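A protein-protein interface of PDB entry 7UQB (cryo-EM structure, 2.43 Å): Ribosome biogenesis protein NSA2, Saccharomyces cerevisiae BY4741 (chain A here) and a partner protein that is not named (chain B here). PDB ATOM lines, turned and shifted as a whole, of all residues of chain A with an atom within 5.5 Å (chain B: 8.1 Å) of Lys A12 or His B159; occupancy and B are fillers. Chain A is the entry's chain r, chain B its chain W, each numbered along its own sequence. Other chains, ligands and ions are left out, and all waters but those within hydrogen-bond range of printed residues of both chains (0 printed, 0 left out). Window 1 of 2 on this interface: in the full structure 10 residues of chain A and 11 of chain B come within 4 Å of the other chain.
Of the printed residues of chain B, Lys A12 touches His B159 and Gly B178.
His B159 touches one residue of chain A.
Printed residues of chain A within 4 Å of Gly B178: Lys A12 (3.5 Å) and Gln A13 (2.9 Å).
Printed residues of chain B within 4 Å of His A14: Ile B175.
Printed residues of chain B within 4 Å of Gln A13: Ile B175 (3.3 Å), Ala B177 (3.3 Å) and Gly B178 (2.9 Å).
Of the printed residues of chain A, Ala B177 touches Gln A13.
Among the printed residues, merely in contact across the chains: Gln A13 with Ile B175, Lys A12 with His B159, Lys A12 with Gly B178, Gly A15 with Ile B175 and His A14 with Ile B175.
Of the 18 printed residues of chain B, 4 touch a printed residue of chain A.
Hydrophobic or aromatic side chains of chain B that line the printed part of chain A: His B159, Ile B175 and Ala B177.
Among the printed residues, 7 pairs touch across the chains.
The side-chain amide nitrogen (NE2) of Gln A13 lies within hydrogen-bond range of the backbone carbonyl oxygen (O) of Ala B177.
The backbone NH of Gly B178 lies within hydrogen-bond range of the backbone carbonyl oxygen of Gln A13 (2.9 Å).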
ATOM      1  N   ILE A   7      -3.700 -15.626   9.700  1.00  0.00           N
ATOM      2  CA  ILE A   7      -4.901 -16.417   9.963  1.00  0.00           C
ATOM      3  C   ILE A   7      -6.148 -15.672   9.497  1.00  0.00           C
ATOM      4  O   ILE A   7      -7.052 -16.266   8.897  1.00  0.00           O
ATOM      5  CB  ILE A   7      -4.978 -16.796  11.454  1.00  0.00           C
ATOM      6  CG1 ILE A   7      -4.015 -17.945  11.763  1.00  0.00           C
ATOM      7  CG2 ILE A   7      -6.395 -17.178  11.858  1.00  0.00           C
ATOM      8  CD1 ILE A   7      -4.380 -19.249  11.085  1.00  0.00           C
ATOM      9  N   GLU A   8      -6.214 -14.361   9.751  1.00  0.00           N
ATOM     10  CA  GLU A   8      -7.338 -13.572   9.258  1.00  0.00           C
ATOM     11  C   GLU A   8      -7.380 -13.562   7.736  1.00  0.00           C
ATOM     12  O   GLU A   8      -8.454 -13.701   7.139  1.00  0.00           O
ATOM     13  CB  GLU A   8      -7.265 -12.145   9.800  1.00  0.00           C
ATOM     14  CG  GLU A   8      -7.960 -11.957  11.134  1.00  0.00           C
ATOM     15  CD  GLU A   8      -7.753 -10.568  11.708  1.00  0.00           C
ATOM     16  OE1 GLU A   8      -7.149  -9.722  11.016  1.00  0.00           O
ATOM     17  OE2 GLU A   8      -8.187 -10.325  12.854  1.00  0.00           O
ATOM     18  N   ARG A   9      -6.219 -13.413   7.090  1.00  0.00           N
ATOM     19  CA  ARG A   9      -6.186 -13.453   5.632  1.00  0.00           C
ATOM     20  C   ARG A   9      -6.565 -14.833   5.102  1.00  0.00           C
ATOM     21  O   ARG A   9      -7.221 -14.942   4.062  1.00  0.00           O
ATOM     22  CB  ARG A   9      -4.808 -13.035   5.116  1.00  0.00           C
ATOM     23  CG  ARG A   9      -4.474 -11.577   5.377  1.00  0.00           C
ATOM     24  CD  ARG A   9      -3.335 -11.089   4.494  1.00  0.00           C
ATOM     25  NE  ARG A   9      -2.202 -12.007   4.485  1.00  0.00           N
ATOM     26  CZ  ARG A   9      -1.255 -12.041   5.412  1.00  0.00           C
ATOM     27  NH1 ARG A   9      -1.284 -11.236   6.459  1.00  0.00           N
ATOM     28  NH2 ARG A   9      -0.253 -12.905   5.282  1.00  0.00           N
ATOM     29  N   HIS A  10      -6.162 -15.896   5.800  1.00  0.00           N
ATOM     30  CA  HIS A  10      -6.525 -17.245   5.380  1.00  0.00           C
ATOM     31  C   HIS A  10      -8.023 -17.478   5.508  1.00  0.00           C
ATOM     32  O   HIS A  10      -8.619 -18.165   4.674  1.00  0.00           O
ATOM     33  CB  HIS A  10      -5.748 -18.277   6.198  1.00  0.00           C
ATOM     34  CG  HIS A  10      -6.138 -19.692   5.910  1.00  0.00           C
ATOM     35  ND1 HIS A  10      -5.526 -20.449   4.935  1.00  0.00           N
ATOM     36  CD2 HIS A  10      -7.084 -20.486   6.464  1.00  0.00           C
ATOM     37  CE1 HIS A  10      -6.078 -21.649   4.902  1.00  0.00           C
ATOM     38  NE2 HIS A  10      -7.026 -21.697   5.819  1.00  0.00           N
ATOM     39  N   ILE A  11      -8.644 -16.935   6.555  1.00  0.00           N
ATOM     40  CA  ILE A  11     -10.097 -17.020   6.675  1.00  0.00           C
ATOM     41  C   ILE A  11     -10.766 -16.208   5.572  1.00  0.00           C
ATOM     42  O   ILE A  11     -11.796 -16.610   5.020  1.00  0.00           O
ATOM     43  CB  ILE A  11     -10.540 -16.569   8.081  1.00  0.00           C
ATOM     44  CG1 ILE A  11     -10.052 -17.568   9.133  1.00  0.00           C
ATOM     45  CG2 ILE A  11     -12.051 -16.416   8.164  1.00  0.00           C
ATOM     46  CD1 ILE A  11     -10.457 -17.221  10.543  1.00  0.00           C
ATOM     47  N   LYS A  12     -10.178 -15.064   5.222  1.00  0.00           N
ATOM     48  CA  LYS A  12     -10.721 -14.231   4.154  1.00  0.00           C
ATOM     49  C   LYS A  12     -10.601 -14.898   2.787  1.00  0.00           C
ATOM     50  O   LYS A  12     -11.445 -14.672   1.914  1.00  0.00           O
ATOM     51  CB  LYS A  12     -10.003 -12.883   4.157  1.00  0.00           C
ATOM     52  CG  LYS A  12     -10.793 -11.728   3.591  1.00  0.00           C
ATOM     53  CD  LYS A  12     -10.319 -10.419   4.199  1.00  0.00           C
ATOM     54  CE  LYS A  12     -10.470 -10.442   5.712  1.00  0.00           C
ATOM     55  NZ  LYS A  12      -9.878  -9.243   6.364  1.00  0.00           N
ATOM     56  N   GLN A  13      -9.568 -15.715   2.584  1.00  0.00           N
ATOM     57  CA  GLN A  13      -9.288 -16.302   1.277  1.00  0.00           C
ATOM     58  C   GLN A  13      -9.869 -17.698   1.096  1.00  0.00           C
ATOM     59  O   GLN A  13     -10.217 -18.070  -0.030  1.00  0.00           O
ATOM     60  CB  GLN A  13      -7.776 -16.365   1.046  1.00  0.00           C
ATOM     61  CG  GLN A  13      -7.129 -15.022   0.769  1.00  0.00           C
ATOM     62  CD  GLN A  13      -7.199 -14.636  -0.692  1.00  0.00           C
ATOM     63  OE1 GLN A  13      -6.565 -15.263  -1.538  1.00  0.00           O
ATOM     64  NE2 GLN A  13      -7.975 -13.606  -0.997  1.00  0.00           N
ATOM     65  N   HIS A  14      -9.968 -18.484   2.167  1.00  0.00           N
ATOM     66  CA  HIS A  14     -10.393 -19.870   2.083  1.00  0.00           C
ATOM     67  C   HIS A  14     -11.634 -20.178   2.901  1.00  0.00           C
ATOM     68  O   HIS A  14     -12.183 -21.278   2.763  1.00  0.00           O
ATOM     69  CB  HIS A  14      -9.262 -20.806   2.539  1.00  0.00           C
ATOM     70  CG  HIS A  14      -7.965 -20.584   1.826  1.00  0.00           C
ATOM     71  ND1 HIS A  14      -7.626 -21.255   0.672  1.00  0.00           N
ATOM     72  CD2 HIS A  14      -6.923 -19.766   2.105  1.00  0.00           C
ATOM     73  CE1 HIS A  14      -6.432 -20.860   0.270  1.00  0.00           C
ATOM     74  NE2 HIS A  14      -5.982 -19.959   1.123  1.00  0.00           N
ATOM     75  N   GLY A  15     -12.092 -19.255   3.738  1.00  0.00           N
ATOM     76  CA  GLY A  15     -13.209 -19.526   4.612  1.00  0.00           C
ATOM     77  C   GLY A  15     -12.792 -20.327   5.830  1.00  0.00           C
ATOM     78  O   GLY A  15     -11.614 -20.426   6.184  1.00  0.00           O
ATOM     79  N   PRO B 156     -17.633  -8.630  -7.479  1.00  0.00           N
ATOM     80  CA  PRO B 156     -17.732  -9.990  -6.934  1.00  0.00           C
ATOM     81  C   PRO B 156     -18.439 -10.010  -5.586  1.00  0.00           C
ATOM     82  O   PRO B 156     -18.333  -9.075  -4.789  1.00  0.00           O
ATOM     83  CB  PRO B 156     -16.269 -10.427  -6.800  1.00  0.00           C
ATOM     84  CG  PRO B 156     -15.535  -9.595  -7.786  1.00  0.00           C
ATOM     85  CD  PRO B 156     -16.246  -8.275  -7.826  1.00  0.00           C
ATOM     86  N   MET B 157     -19.169 -11.095  -5.344  1.00  0.00           N
ATOM     87  CA  MET B 157     -19.875 -11.268  -4.081  1.00  0.00           C
ATOM     88  C   MET B 157     -18.882 -11.388  -2.933  1.00  0.00           C
ATOM     89  O   MET B 157     -17.831 -12.020  -3.064  1.00  0.00           O
ATOM     90  CB  MET B 157     -20.765 -12.508  -4.139  1.00  0.00           C
ATOM     91  CG  MET B 157     -21.662 -12.701  -2.928  1.00  0.00           C
ATOM     92  SD  MET B 157     -23.372 -12.229  -3.245  1.00  0.00           S
ATOM     93  CE  MET B 157     -23.862 -13.503  -4.401  1.00  0.00           C
ATOM     94  N   ILE B 158     -19.218 -10.766  -1.801  1.00  0.00           N
ATOM     95  CA  ILE B 158     -18.326 -10.771  -0.649  1.00  0.00           C
ATOM     96  C   ILE B 158     -18.212 -12.188  -0.097  1.00  0.00           C
ATOM     97  O   ILE B 158     -19.171 -12.972  -0.131  1.00  0.00           O
ATOM     98  CB  ILE B 158     -18.818  -9.771   0.415  1.00  0.00           C
ATOM     99  CG1 ILE B 158     -17.790  -9.609   1.537  1.00  0.00           C
ATOM    100  CG2 ILE B 158     -20.167 -10.185   0.976  1.00  0.00           C
ATOM    101  CD1 ILE B 158     -16.442  -9.122   1.063  1.00  0.00           C
ATOM    102  N   HIS B 159     -17.013 -12.536   0.377  1.00  0.00           N
ATOM    103  CA  HIS B 159     -16.750 -13.877   0.885  1.00  0.00           C
ATOM    104  C   HIS B 159     -17.563 -14.206   2.129  1.00  0.00           C
ATOM    105  O   HIS B 159     -17.751 -15.387   2.435  1.00  0.00           O
ATOM    106  CB  HIS B 159     -15.262 -14.023   1.195  1.00  0.00           C
ATOM    107  CG  HIS B 159     -14.795 -13.138   2.306  1.00  0.00           C
ATOM    108  ND1 HIS B 159     -14.751 -13.553   3.620  1.00  0.00           N
ATOM    109  CD2 HIS B 159     -14.379 -11.850   2.305  1.00  0.00           C
ATOM    110  CE1 HIS B 159     -14.313 -12.564   4.377  1.00  0.00           C
ATOM    111  NE2 HIS B 159     -14.082 -11.518   3.604  1.00  0.00           N
ATOM    112  N   SER B 160     -18.045 -13.191   2.853  1.00  0.00           N
ATOM    113  CA  SER B 160     -18.805 -13.429   4.074  1.00  0.00           C
ATOM    114  C   SER B 160     -20.174 -14.037   3.805  1.00  0.00           C
ATOM    115  O   SER B 160     -20.788 -14.579   4.730  1.00  0.00           O
ATOM    116  CB  SER B 160     -18.964 -12.122   4.853  1.00  0.00           C
ATOM    117  OG  SER B 160     -17.710 -11.504   5.074  1.00  0.00           O
ATOM    118  N   LEU B 161     -20.668 -13.956   2.573  1.00  0.00           N
ATOM    119  CA  LEU B 161     -21.973 -14.501   2.229  1.00  0.00           C
ATOM    120  C   LEU B 161     -21.925 -15.959   1.797  1.00  0.00           C
ATOM    121  O   LEU B 161     -22.986 -16.564   1.609  1.00  0.00           O
ATOM    122  CB  LEU B 161     -22.614 -13.669   1.115  1.00  0.00           C
ATOM    123  CG  LEU B 161     -23.216 -12.331   1.543  1.00  0.00           C
ATOM    124  CD1 LEU B 161     -23.633 -11.524   0.329  1.00  0.00           C
ATOM    125  CD2 LEU B 161     -24.398 -12.555   2.473  1.00  0.00           C
ATOM    126  N   GLU B 162     -20.734 -16.532   1.629  1.00  0.00           N
ATOM    127  CA  GLU B 162     -20.638 -17.921   1.191  1.00  0.00           C
ATOM    128  C   GLU B 162     -21.255 -18.923   2.167  1.00  0.00           C
ATOM    129  O   GLU B 162     -21.914 -19.862   1.689  1.00  0.00           O
ATOM    130  CB  GLU B 162     -19.176 -18.272   0.881  1.00  0.00           C
ATOM    131  CG  GLU B 162     -19.014 -19.415  -0.112  1.00  0.00           C
ATOM    132  CD  GLU B 162     -19.000 -20.775   0.556  1.00  0.00           C
ATOM    133  OE1 GLU B 162     -18.693 -20.842   1.764  1.00  0.00           O
ATOM    134  OE2 GLU B 162     -19.296 -21.779  -0.124  1.00  0.00           O
ATOM    135  N   PRO B 163     -21.071 -18.828   3.497  1.00  0.00           N
ATOM    136  CA  PRO B 163     -21.828 -19.736   4.380  1.00  0.00           C
ATOM    137  C   PRO B 163     -23.336 -19.604   4.246  1.00  0.00           C
ATOM    138  O   PRO B 163     -24.045 -20.614   4.318  1.00  0.00           O
ATOM    139  CB  PRO B 163     -21.347 -19.338   5.781  1.00  0.00           C
ATOM    140  CG  PRO B 163     -19.991 -18.803   5.561  1.00  0.00           C
ATOM    141  CD  PRO B 163     -20.065 -18.067   4.264  1.00  0.00           C
ATOM    142  N   THR B 164     -23.846 -18.386   4.046  1.00  0.00           N
ATOM    143  CA  THR B 164     -25.283 -18.204   3.859  1.00  0.00           C
ATOM    144  C   THR B 164     -25.762 -18.853   2.565  1.00  0.00           C
ATOM    145  O   THR B 164     -26.799 -19.527   2.550  1.00  0.00           O
ATOM    146  CB  THR B 164     -25.628 -16.714   3.877  1.00  0.00           C
ATOM    147  OG1 THR B 164     -25.383 -16.183   5.185  1.00  0.00           O
ATOM    148  CG2 THR B 164     -27.087 -16.486   3.514  1.00  0.00           C
ATOM    149  N   MET B 165     -25.015 -18.674   1.474  1.00  0.00           N
ATOM    150  CA  MET B 165     -25.402 -19.276   0.203  1.00  0.00           C
ATOM    151  C   MET B 165     -25.309 -20.796   0.256  1.00  0.00           C
ATOM    152  O   MET B 165     -26.138 -21.494  -0.338  1.00  0.00           O
ATOM    153  CB  MET B 165     -24.530 -18.732  -0.927  1.00  0.00           C
ATOM    154  CG  MET B 165     -24.631 -17.233  -1.133  1.00  0.00           C
ATOM    155  SD  MET B 165     -23.639 -16.665  -2.525  1.00  0.00           S
ATOM    156  CE  MET B 165     -24.562 -17.338  -3.904  1.00  0.00           C
ATOM    157  N   ARG B 166     -24.303 -21.325   0.950  1.00  0.00           N
ATOM    158  CA  ARG B 166     -24.103 -22.768   0.991  1.00  0.00           C
ATOM    159  C   ARG B 166     -25.093 -23.457   1.923  1.00  0.00           C
ATOM    160  O   ARG B 166     -25.586 -24.545   1.608  1.00  0.00           O
ATOM    161  CB  ARG B 166     -22.667 -23.082   1.412  1.00  0.00           C
ATOM    162  CG  ARG B 166     -22.258 -24.524   1.179  1.00  0.00           C
ATOM    163  CD  ARG B 166     -20.844 -24.798   1.665  1.00  0.00           C
ATOM    164  NE  ARG B 166     -20.718 -24.637   3.109  1.00  0.00           N
ATOM    165  CZ  ARG B 166     -20.037 -23.664   3.699  1.00  0.00           C
ATOM    166  NH1 ARG B 166     -19.387 -22.753   2.997  1.00  0.00           N
ATOM    167  NH2 ARG B 166     -20.003 -23.609   5.026  1.00  0.00           N
ATOM    168  N   LYS B 174     -18.073 -22.747  -3.562  1.00  0.00           N
ATOM    169  CA  LYS B 174     -16.723 -22.901  -3.053  1.00  0.00           C
ATOM    170  C   LYS B 174     -16.095 -21.522  -2.931  1.00  0.00           C
ATOM    171  O   LYS B 174     -16.534 -20.560  -3.563  1.00  0.00           O
ATOM    172  CB  LYS B 174     -15.853 -23.787  -3.963  1.00  0.00           C
ATOM    173  CG  LYS B 174     -16.152 -25.277  -3.897  1.00  0.00           C
ATOM    174  CD  LYS B 174     -17.316 -25.663  -4.798  1.00  0.00           C
ATOM    175  CE  LYS B 174     -17.606 -27.150  -4.727  1.00  0.00           C
ATOM    176  NZ  LYS B 174     -18.874 -27.494  -5.429  1.00  0.00           N
ATOM    177  N   ILE B 175     -15.063 -21.433  -2.100  1.00  0.00           N
ATOM    178  CA  ILE B 175     -14.272 -20.218  -1.960  1.00  0.00           C
ATOM    179  C   ILE B 175     -12.931 -20.465  -2.635  1.00  0.00           C
ATOM    180  O   ILE B 175     -12.214 -21.409  -2.282  1.00  0.00           O
ATOM    181  CB  ILE B 175     -14.092 -19.819  -0.488  1.00  0.00           C
ATOM    182  CG1 ILE B 175     -15.442 -19.824   0.227  1.00  0.00           C
ATOM    183  CG2 ILE B 175     -13.456 -18.446  -0.390  1.00  0.00           C
ATOM    184  CD1 ILE B 175     -15.389 -19.331   1.654  1.00  0.00           C
ATOM    185  N   LYS B 176     -12.603 -19.627  -3.615  1.00  0.00           N
ATOM    186  CA  LYS B 176     -11.349 -19.708  -4.356  1.00  0.00           C
ATOM    187  C   LYS B 176     -10.726 -18.321  -4.378  1.00  0.00           C
ATOM    188  O   LYS B 176     -11.279 -17.403  -4.997  1.00  0.00           O
ATOM    189  CB  LYS B 176     -11.574 -20.224  -5.777  1.00  0.00           C
ATOM    190  CG  LYS B 176     -11.914 -21.700  -5.868  1.00  0.00           C
ATOM    191  CD  LYS B 176     -11.997 -22.145  -7.320  1.00  0.00           C
ATOM    192  CE  LYS B 176     -12.244 -23.638  -7.430  1.00  0.00           C
ATOM    193  NZ  LYS B 176     -13.490 -24.043  -6.726  1.00  0.00           N
ATOM    194  N   ALA B 177      -9.585 -18.176  -3.698  1.00  0.00           N
ATOM    195  CA  ALA B 177      -8.853 -16.910  -3.602  1.00  0.00           C
ATOM    196  C   ALA B 177      -9.759 -15.777  -3.125  1.00  0.00           C
ATOM    197  O   ALA B 177      -9.707 -14.654  -3.630  1.00  0.00           O
ATOM    198  CB  ALA B 177      -8.185 -16.556  -4.933  1.00  0.00           C
ATOM    199  N   GLY B 178     -10.607 -16.082  -2.147  1.00  0.00           N
ATOM    200  CA  GLY B 178     -11.522 -15.102  -1.605  1.00  0.00           C
ATOM    201  C   GLY B 178     -12.719 -14.783  -2.468  1.00  0.00           C
ATOM    202  O   GLY B 178     -13.388 -13.775  -2.217  1.00  0.00           O
ATOM    203  N   LYS B 179     -13.016 -15.600  -3.476  1.00  0.00           N
ATOM    204  CA  LYS B 179     -14.152 -15.372  -4.358  1.00  0.00           C
ATOM    205  C   LYS B 179     -15.096 -16.566  -4.309  1.00  0.00           C
ATOM    206  O   LYS B 179     -14.655 -17.711  -4.196  1.00  0.00           O
ATOM    207  CB  LYS B 179     -13.692 -15.125  -5.797  1.00  0.00           C
ATOM    208  CG  LYS B 179     -12.876 -13.855  -5.962  1.00  0.00           C
ATOM    209  CD  LYS B 179     -12.409 -13.677  -7.390  1.00  0.00           C
ATOM    210  CE  LYS B 179     -11.725 -12.334  -7.575  1.00  0.00           C
ATOM    211  NZ  LYS B 179     -11.291 -12.127  -8.982  1.00  0.00           N
ATOM    212  N   ILE B 180     -16.394 -16.294  -4.390  1.00  0.00           N
ATOM    213  CA  ILE B 180     -17.391 -17.357  -4.399  1.00  0.00           C
ATOM    214  C   ILE B 180     -17.522 -17.901  -5.815  1.00  0.00           C
ATOM    215  O   ILE B 180     -17.631 -17.136  -6.781  1.00  0.00           O
ATOM    216  CB  ILE B 180     -18.740 -16.849  -3.865  1.00  0.00           C
ATOM    217  CG1 ILE B 180     -18.566 -16.259  -2.467  1.00  0.00           C
ATOM    218  CG2 ILE B 180     -19.759 -17.974  -3.834  1.00  0.00           C
ATOM    219  CD1 ILE B 180     -19.852 -15.756  -1.855  1.00  0.00           C
